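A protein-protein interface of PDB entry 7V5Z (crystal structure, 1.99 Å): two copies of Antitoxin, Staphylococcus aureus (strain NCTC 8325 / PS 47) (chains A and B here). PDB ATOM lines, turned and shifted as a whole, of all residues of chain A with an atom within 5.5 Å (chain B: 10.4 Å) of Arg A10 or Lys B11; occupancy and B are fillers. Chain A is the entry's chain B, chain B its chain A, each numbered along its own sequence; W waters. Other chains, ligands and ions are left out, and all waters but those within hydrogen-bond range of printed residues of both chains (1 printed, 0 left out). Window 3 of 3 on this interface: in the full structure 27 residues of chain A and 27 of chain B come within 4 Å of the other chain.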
ATOM      1  N   SER A   5      24.024 -12.759  16.288  1.00  0.00           N
ATOM      2  CA  SER A   5      23.433 -12.178  15.095  1.00  0.00           C
ATOM      3  C   SER A   5      22.051 -12.776  14.837  1.00  0.00           C
ATOM      4  O   SER A   5      21.723 -13.856  15.349  1.00  0.00           O
ATOM      5  CB  SER A   5      24.338 -12.421  13.896  1.00  0.00           C
ATOM      6  OG  SER A   5      24.076 -13.708  13.395  1.00  0.00           O
ATOM      7  N   PRO A   6      21.207 -12.082  14.057  1.00  0.00           N
ATOM      8  CA  PRO A   6      19.871 -12.630  13.756  1.00  0.00           C
ATOM      9  C   PRO A   6      19.919 -14.014  13.138  1.00  0.00           C
ATOM     10  O   PRO A   6      19.085 -14.873  13.451  1.00  0.00           O
ATOM     11  CB  PRO A   6      19.291 -11.602  12.785  1.00  0.00           C
ATOM     12  CG  PRO A   6      20.024 -10.354  13.082  1.00  0.00           C
ATOM     13  CD  PRO A   6      21.400 -10.751  13.459  1.00  0.00           C
ATOM     14  N   THR A   7      20.908 -14.260  12.283  1.00  0.00           N
ATOM     15  CA  THR A   7      20.996 -15.549  11.609  1.00  0.00           C
ATOM     16  C   THR A   7      21.479 -16.648  12.549  1.00  0.00           C
ATOM     17  O   THR A   7      20.966 -17.771  12.510  1.00  0.00           O
ATOM     18  CB  THR A   7      21.902 -15.406  10.389  1.00  0.00           C
ATOM     19  OG1 THR A   7      21.214 -14.588   9.429  1.00  0.00           O
ATOM     20  CG2 THR A   7      22.254 -16.792   9.778  1.00  0.00           C
ATOM     21  N   GLU A   8      22.474 -16.354  13.396  1.00  0.00           N
ATOM     22  CA  GLU A   8      22.920 -17.341  14.379  1.00  0.00           C
ATOM     23  C   GLU A   8      21.818 -17.649  15.386  1.00  0.00           C
ATOM     24  O   GLU A   8      21.652 -18.802  15.806  1.00  0.00           O
ATOM     25  CB  GLU A   8      24.163 -16.840  15.116  1.00  0.00           C
ATOM     26  CG  GLU A   8      25.353 -16.548  14.229  1.00  0.00           C
ATOM     27  CD  GLU A   8      26.535 -15.957  14.999  1.00  0.00           C
ATOM     28  OE1 GLU A   8      27.610 -16.607  15.012  1.00  0.00           O
ATOM     29  OE2 GLU A   8      26.393 -14.845  15.576  1.00  0.00           O
ATOM     30  N   ALA A   9      21.069 -16.622  15.799  1.00  0.00           N
ATOM     31  CA  ALA A   9      19.971 -16.835  16.734  1.00  0.00           C
ATOM     32  C   ALA A   9      18.914 -17.739  16.121  1.00  0.00           C
ATOM     33  O   ALA A   9      18.396 -18.644  16.788  1.00  0.00           O
ATOM     34  CB  ALA A   9      19.360 -15.494  17.142  1.00  0.00           C
ATOM     35  N   ARG A  10      18.593 -17.521  14.846  1.00  0.00           N
ATOM     36  CA  ARG A  10      17.626 -18.376  14.170  1.00  0.00           C
ATOM     37  C   ARG A  10      18.116 -19.812  14.101  1.00  0.00           C
ATOM     38  O   ARG A  10      17.350 -20.749  14.347  1.00  0.00           O
ATOM     39  CB  ARG A  10      17.341 -17.841  12.770  1.00  0.00           C
ATOM     40  CG  ARG A  10      16.142 -18.496  12.119  1.00  0.00           C
ATOM     41  CD  ARG A  10      16.036 -18.175  10.620  1.00  0.00           C
ATOM     42  NE  ARG A  10      14.851 -18.822  10.072  1.00  0.00           N
ATOM     43  CZ  ARG A  10      14.852 -19.731   9.107  1.00  0.00           C
ATOM     44  NH1 ARG A  10      15.988 -20.104   8.525  1.00  0.00           N
ATOM     45  NH2 ARG A  10      13.697 -20.251   8.704  1.00  0.00           N
ATOM     46  N   LYS A  11      19.395 -20.002  13.779  1.00  0.00           N
ATOM     47  CA  LYS A  11      19.935 -21.347  13.619  1.00  0.00           C
ATOM     48  C   LYS A  11      19.914 -22.127  14.932  1.00  0.00           C
ATOM     49  O   LYS A  11      19.552 -23.310  14.952  1.00  0.00           O
ATOM     50  CB  LYS A  11      21.356 -21.265  13.063  1.00  0.00           C
ATOM     51  CG  LYS A  11      21.917 -22.605  12.648  1.00  0.00           C
ATOM     52  CD  LYS A  11      23.436 -22.610  12.637  1.00  0.00           C
ATOM     53  CE  LYS A  11      24.003 -23.149  13.943  1.00  0.00           C
ATOM     54  NZ  LYS A  11      25.425 -22.739  14.129  1.00  0.00           N
ATOM     55  N   ASP A  12      20.295 -21.482  16.039  1.00  0.00           N
ATOM     56  CA  ASP A  12      20.376 -22.121  17.347  1.00  0.00           C
ATOM     57  C   ASP A  12      19.218 -21.711  18.263  1.00  0.00           C
ATOM     58  O   ASP A  12      19.368 -21.672  19.487  1.00  0.00           O
ATOM     59  CB  ASP A  12      21.722 -21.810  18.004  1.00  0.00           C
ATOM     60  CG  ASP A  12      22.241 -22.975  18.860  1.00  0.00           C
ATOM     61  OD1 ASP A  12      23.159 -22.748  19.675  1.00  0.00           O
ATOM     62  OD2 ASP A  12      21.726 -24.115  18.731  1.00  0.00           O
ATOM     63  N   PHE A  13      18.044 -21.454  17.675  1.00  0.00           N
ATOM     64  CA  PHE A  13      16.929 -20.854  18.401  1.00  0.00           C
ATOM     65  C   PHE A  13      16.486 -21.698  19.592  1.00  0.00           C
ATOM     66  O   PHE A  13      16.212 -21.161  20.672  1.00  0.00           O
ATOM     67  CB  PHE A  13      15.756 -20.640  17.444  1.00  0.00           C
ATOM     68  CG  PHE A  13      14.647 -19.796  18.020  1.00  0.00           C
ATOM     69  CD1 PHE A  13      14.896 -18.504  18.448  1.00  0.00           C
ATOM     70  CD2 PHE A  13      13.361 -20.295  18.122  1.00  0.00           C
ATOM     71  CE1 PHE A  13      13.882 -17.721  18.967  1.00  0.00           C
ATOM     72  CE2 PHE A  13      12.349 -19.520  18.638  1.00  0.00           C
ATOM     73  CZ  PHE A  13      12.609 -18.229  19.060  1.00  0.00           C
ATOM     74  N   THR B   4       3.252 -17.154  19.964  1.00  0.00           N
ATOM     75  CA  THR B   4       3.626 -18.075  18.907  1.00  0.00           C
ATOM     76  C   THR B   4       4.423 -19.211  19.524  1.00  0.00           C
ATOM     77  O   THR B   4       4.906 -19.108  20.651  1.00  0.00           O
ATOM     78  CB  THR B   4       4.421 -17.360  17.816  1.00  0.00           C
ATOM     79  OG1 THR B   4       4.718 -18.278  16.759  1.00  0.00           O
ATOM     80  CG2 THR B   4       5.709 -16.806  18.393  1.00  0.00           C
ATOM     81  N   SER B   5       4.544 -20.297  18.790  1.00  0.00           N
ATOM     82  CA  SER B   5       5.293 -21.437  19.298  1.00  0.00           C
ATOM     83  C   SER B   5       6.772 -21.278  18.981  1.00  0.00           C
ATOM     84  O   SER B   5       7.143 -20.479  18.116  1.00  0.00           O
ATOM     85  CB  SER B   5       4.765 -22.724  18.675  1.00  0.00           C
ATOM     86  OG  SER B   5       5.263 -22.852  17.357  1.00  0.00           O
ATOM     87  N   PRO B   6       7.652 -22.013  19.672  1.00  0.00           N
ATOM     88  CA  PRO B   6       9.067 -22.023  19.255  1.00  0.00           C
ATOM     89  C   PRO B   6       9.240 -22.387  17.790  1.00  0.00           C
ATOM     90  O   PRO B   6      10.018 -21.744  17.074  1.00  0.00           O
ATOM     91  CB  PRO B   6       9.696 -23.074  20.178  1.00  0.00           C
ATOM     92  CG  PRO B   6       8.804 -23.113  21.371  1.00  0.00           C
ATOM     93  CD  PRO B   6       7.419 -22.868  20.850  1.00  0.00           C
ATOM     94  N   THR B   7       8.520 -23.407  17.324  1.00  0.00           N
ATOM     95  CA  THR B   7       8.669 -23.846  15.938  1.00  0.00           C
ATOM     96  C   THR B   7       8.289 -22.744  14.957  1.00  0.00           C
ATOM     97  O   THR B   7       9.040 -22.445  14.025  1.00  0.00           O
ATOM     98  CB  THR B   7       7.823 -25.093  15.681  1.00  0.00           C
ATOM     99  OG1 THR B   7       8.265 -26.150  16.546  1.00  0.00           O
ATOM    100  CG2 THR B   7       7.992 -25.526  14.225  1.00  0.00           C
ATOM    101  N   GLU B   8       7.115 -22.130  15.144  1.00  0.00           N
ATOM    102  CA  GLU B   8       6.692 -21.091  14.212  1.00  0.00           C
ATOM    103  C   GLU B   8       7.564 -19.849  14.332  1.00  0.00           C
ATOM    104  O   GLU B   8       7.852 -19.193  13.328  1.00  0.00           O
ATOM    105  CB  GLU B   8       5.218 -20.749  14.432  1.00  0.00           C
ATOM    106  CG  GLU B   8       4.308 -21.971  14.454  1.00  0.00           C
ATOM    107  CD  GLU B   8       2.946 -21.686  15.072  1.00  0.00           C
ATOM    108  OE1 GLU B   8       1.926 -21.936  14.390  1.00  0.00           O
ATOM    109  OE2 GLU B   8       2.896 -21.202  16.230  1.00  0.00           O
ATOM    110  N   ALA B   9       7.995 -19.512  15.552  1.00  0.00           N
ATOM    111  CA  ALA B   9       8.859 -18.350  15.727  1.00  0.00           C
ATOM    112  C   ALA B   9      10.156 -18.511  14.952  1.00  0.00           C
ATOM    113  O   ALA B   9      10.650 -17.551  14.350  1.00  0.00           O
ATOM    114  CB  ALA B   9       9.158 -18.126  17.208  1.00  0.00           C
ATOM    115  N   ARG B  10      10.735 -19.716  14.978  1.00  0.00           N
ATOM    116  CA  ARG B  10      11.991 -19.948  14.272  1.00  0.00           C
ATOM    117  C   ARG B  10      11.806 -19.824  12.764  1.00  0.00           C
ATOM    118  O   ARG B  10      12.665 -19.259  12.076  1.00  0.00           O
ATOM    119  CB  ARG B  10      12.553 -21.326  14.629  1.00  0.00           C
ATOM    120  CG  ARG B  10      13.927 -21.612  14.026  1.00  0.00           C
ATOM    121  CD  ARG B  10      14.557 -22.902  14.600  1.00  0.00           C
ATOM    122  NE  ARG B  10      15.086 -23.764  13.548  1.00  0.00           N
ATOM    123  CZ  ARG B  10      16.372 -23.885  13.236  1.00  0.00           C
ATOM    124  NH1 ARG B  10      16.741 -24.692  12.253  1.00  0.00           N
ATOM    125  NH2 ARG B  10      17.296 -23.214  13.907  1.00  0.00           N
ATOM    126  N   LYS B  11      10.697 -20.346  12.227  1.00  0.00           N
ATOM    127  CA  LYS B  11      10.460 -20.216  10.788  1.00  0.00           C
ATOM    128  C   LYS B  11      10.210 -18.765  10.389  1.00  0.00           C
ATOM    129  O   LYS B  11      10.677 -18.319   9.337  1.00  0.00           O
ATOM    130  CB  LYS B  11       9.298 -21.113  10.351  1.00  0.00           C
ATOM    131  CG  LYS B  11       9.550 -22.587  10.645  1.00  0.00           C
ATOM    132  CD  LYS B  11       8.583 -23.513   9.919  1.00  0.00           C
ATOM    133  CE  LYS B  11       7.143 -23.078  10.124  1.00  0.00           C
ATOM    134  NZ  LYS B  11       6.252 -24.243  10.403  1.00  0.00           N
ATOM    135  N   ASP B  12       9.496 -18.003  11.222  1.00  0.00           N
ATOM    136  CA  ASP B  12       9.163 -16.617  10.915  1.00  0.00           C
ATOM    137  C   ASP B  12      10.087 -15.620  11.606  1.00  0.00           C
ATOM    138  O   ASP B  12       9.703 -14.465  11.807  1.00  0.00           O
ATOM    139  CB  ASP B  12       7.712 -16.336  11.288  1.00  0.00           C
ATOM    140  CG  ASP B  12       6.764 -16.647  10.152  1.00  0.00           C
ATOM    141  OD1 ASP B  12       6.323 -17.815  10.036  1.00  0.00           O
ATOM    142  OD2 ASP B  12       6.479 -15.720   9.360  1.00  0.00           O
ATOM    143  N   PHE B  13      11.316 -16.039  11.917  1.00  0.00           N
ATOM    144  CA  PHE B  13      12.157 -15.283  12.839  1.00  0.00           C
ATOM    145  C   PHE B  13      12.502 -13.899  12.301  1.00  0.00           C
ATOM    146  O   PHE B  13      12.500 -12.917  13.051  1.00  0.00           O
ATOM    147  CB  PHE B  13      13.425 -16.082  13.155  1.00  0.00           C
ATOM    148  CG  PHE B  13      14.201 -15.549  14.325  1.00  0.00           C
ATOM    149  CD1 PHE B  13      13.678 -15.600  15.607  1.00  0.00           C
ATOM    150  CD2 PHE B  13      15.444 -14.977  14.141  1.00  0.00           C
ATOM    151  CE1 PHE B  13      14.394 -15.099  16.694  1.00  0.00           C
ATOM    152  CE2 PHE B  13      16.164 -14.477  15.216  1.00  0.00           C
ATOM    153  CZ  PHE B  13      15.636 -14.534  16.492  1.00  0.00           C
ATOM    154  N   TYR B  14      12.813 -13.790  11.010  1.00  0.00           N
ATOM    155  CA  TYR B  14      13.242 -12.488  10.506  1.00  0.00           C
ATOM    156  C   TYR B  14      12.091 -11.489  10.531  1.00  0.00           C
ATOM    157  O   TYR B  14      12.282 -10.321  10.885  1.00  0.00           O
ATOM    158  CB  TYR B  14      13.826 -12.634   9.101  1.00  0.00           C
ATOM    159  CG  TYR B  14      15.143 -13.398   9.097  1.00  0.00           C
ATOM    160  CD1 TYR B  14      16.236 -12.923   9.804  1.00  0.00           C
ATOM    161  CD2 TYR B  14      15.285 -14.603   8.401  1.00  0.00           C
ATOM    162  CE1 TYR B  14      17.447 -13.612   9.816  1.00  0.00           C
ATOM    163  CE2 TYR B  14      16.505 -15.305   8.402  1.00  0.00           C
ATOM    164  CZ  TYR B  14      17.576 -14.797   9.112  1.00  0.00           C
ATOM    165  OH  TYR B  14      18.783 -15.461   9.137  1.00  0.00           O
ATOM    166  N   GLN B  15      10.887 -11.931  10.179  1.00  0.00           N
ATOM    167  CA  GLN B  15       9.732 -11.044  10.224  1.00  0.00           C
ATOM    168  C   GLN B  15       9.359 -10.698  11.658  1.00  0.00           C
ATOM    169  O   GLN B  15       8.934  -9.569  11.934  1.00  0.00           O
ATOM    170  CB  GLN B  15       8.551 -11.693   9.495  1.00  0.00           C
ATOM    171  CG  GLN B  15       7.343 -10.774   9.343  1.00  0.00           C
ATOM    172  CD  GLN B  15       7.679  -9.528   8.547  1.00  0.00           C
ATOM    173  OE1 GLN B  15       8.421  -9.590   7.568  1.00  0.00           O
ATOM    174  NE2 GLN B  15       7.146  -8.390   8.969  1.00  0.00           N
ATOM    175  N   LEU B  16       9.516 -11.657  12.576  1.00  0.00           N
ATOM    176  CA  LEU B  16       9.238 -11.405  13.987  1.00  0.00           C
ATOM    177  C   LEU B  16      10.096 -10.265  14.510  1.00  0.00           C
ATOM    178  O   LEU B  16       9.604  -9.394  15.236  1.00  0.00           O
ATOM    179  CB  LEU B  16       9.492 -12.665  14.814  1.00  0.00           C
ATOM    180  CG  LEU B  16       8.541 -13.860  14.799  1.00  0.00           C
ATOM    181  CD1 LEU B  16       8.689 -14.617  16.130  1.00  0.00           C
ATOM    182  CD2 LEU B  16       7.080 -13.448  14.524  1.00  0.00           C
ATOM    183  N   LEU B  17      11.394 -10.268  14.159  1.00  0.00           N
ATOM    184  CA  LEU B  17      12.298  -9.214  14.613  1.00  0.00           C
ATOM    185  C   LEU B  17      11.865  -7.853  14.086  1.00  0.00           C
ATOM    186  O   LEU B  17      11.892  -6.858  14.822  1.00  0.00           O
ATOM    187  CB  LEU B  17      13.735  -9.516  14.181  1.00  0.00           C
ATOM    188  CG  LEU B  17      14.337 -10.774  14.802  1.00  0.00           C
ATOM    189  CD1 LEU B  17      15.739 -11.073  14.265  1.00  0.00           C
ATOM    190  CD2 LEU B  17      14.381 -10.602  16.299  1.00  0.00           C
ATOM    191  N   ILE B  29       6.957 -16.382  23.145  1.00  0.00           N
ATOM    192  CA  ILE B  29       7.274 -17.715  22.660  1.00  0.00           C
ATOM    193  C   ILE B  29       6.800 -18.678  23.736  1.00  0.00           C
ATOM    194  O   ILE B  29       7.352 -18.702  24.838  1.00  0.00           O
ATOM    195  CB  ILE B  29       8.773 -17.884  22.399  1.00  0.00           C
ATOM    196  CG1 ILE B  29       9.359 -16.681  21.640  1.00  0.00           C
ATOM    197  CG2 ILE B  29       9.049 -19.216  21.719  1.00  0.00           C
ATOM    198  CD1 ILE B  29       8.718 -16.392  20.308  1.00  0.00           C
ATOM    199  N   ILE B  40      10.390 -12.042  23.210  1.00  0.00           N
ATOM    200  CA  ILE B  40      11.271 -11.279  22.337  1.00  0.00           C
ATOM    201  C   ILE B  40      10.755  -9.856  22.314  1.00  0.00           C
ATOM    202  O   ILE B  40       9.550  -9.637  22.161  1.00  0.00           O
ATOM    203  CB  ILE B  40      11.333 -11.884  20.926  1.00  0.00           C
ATOM    204  CG1 ILE B  40      12.009 -13.258  21.011  1.00  0.00           C
ATOM    205  CG2 ILE B  40      12.107 -10.987  20.017  1.00  0.00           C
ATOM    206  CD1 ILE B  40      12.035 -14.028  19.699  1.00  0.00           C
HETATM  207  O   HOH W   1      17.475 -24.270  16.702  1.00  0.00           O
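The guanidinium group of Arg B10 lies within hydrogen-bond range of the backbone carbonyl oxygen of Arg A10 (2.5 Å). The backbone carbonyl oxygen (O) of Lys A11 lies within hydrogen-bond range of the guanidinium group (NH2) of Arg B10. OH of Tyr B14 lies within hydrogen-bond range of OG1 of Thr A7.
The side-chain hydroxyl (OG) of Ser A5 sits close to the backbone NH (N) of Thr A7.
Among the printed residues, merely in contact across the chains: Pro A6 with Phe B13 (3.4 Å), Phe A13 with Phe B13 (3.5 Å), Phe A13 with Pro B6 (3.6 Å), Arg A10 with Lys B11 (3.6 Å), Arg A10 with Tyr B14 (3.7 Å), Arg A10 with Phe B13 (3.7 Å), Phe A13 with Arg B10 (3.7 Å), Phe A13 with Ala B9 (3.8 Å), Ala A9 with Phe B13 (3.9 Å) and Pro A6 with Leu B17 (3.9 Å).
Of the printed residues of chain B, Pro A6 touches Phe B13 and Leu B17. Of chain B, only Tyr B14 (2.6 Å) comes within 4 Å of Thr A7. Of chain B, only Phe B13 comes within 4 Å of Ala A9. Of chain B, only Arg B10, Lys B11, Phe B13 and Tyr B14 come within 4 Å of Arg A10. Of the printed residues of chain B, Phe A13 touches Pro B6 (3.6 Å), Ala B9 (3.8 Å), Arg B10 (3.7 Å) and Phe B13 (3.5 Å). Of the printed residues of chain A, Pro B6 touches Phe A13. Printed residues of chain A within 4 Å of Arg B10: Arg A10, Lys A11 and Phe A13. The nearest residue of chain B that does not touch Arg A10 is Asp B12 (5.4 Å). The nearest printed residue of chain A that does not touch Lys B11 is Phe A13 (6.5 Å).
Of the 16 printed residues of chain B, 7 touch a printed residue of chain A. Printed residues of chain B that touch a printed residue of chain A: Pro B6, Ala B9, Arg B10, Lys B11, Phe B13, Tyr B14 and Leu B17. Hydrophobic or aromatic side chains of chain B that line the printed part of chain A: Ala B9, Phe B13, Tyr B14 and Leu B17. Among the printed residues, 13 pairs touch across the chains.
Ala A9 touches Phe B13, and with the chains exchanged Phe A13 touches Ala B9. Arg A10 touches its own counterpart, Arg B10. Arg A10 touches Lys B11, and with the chains exchanged Lys A11 touches Arg B10. Arg A10 touches Phe B13, and with the chains exchanged Phe A13 touches Arg B10. 9 positions are printed for both chains. Of the 13 pairs that touch across the chains among the printed residues, 10 have their exchanged pair printed and touching as well.
Water W1 lies within hydrogen-bond range of O of Lys A11, NH2 of Arg B10 and N of Phe A13.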
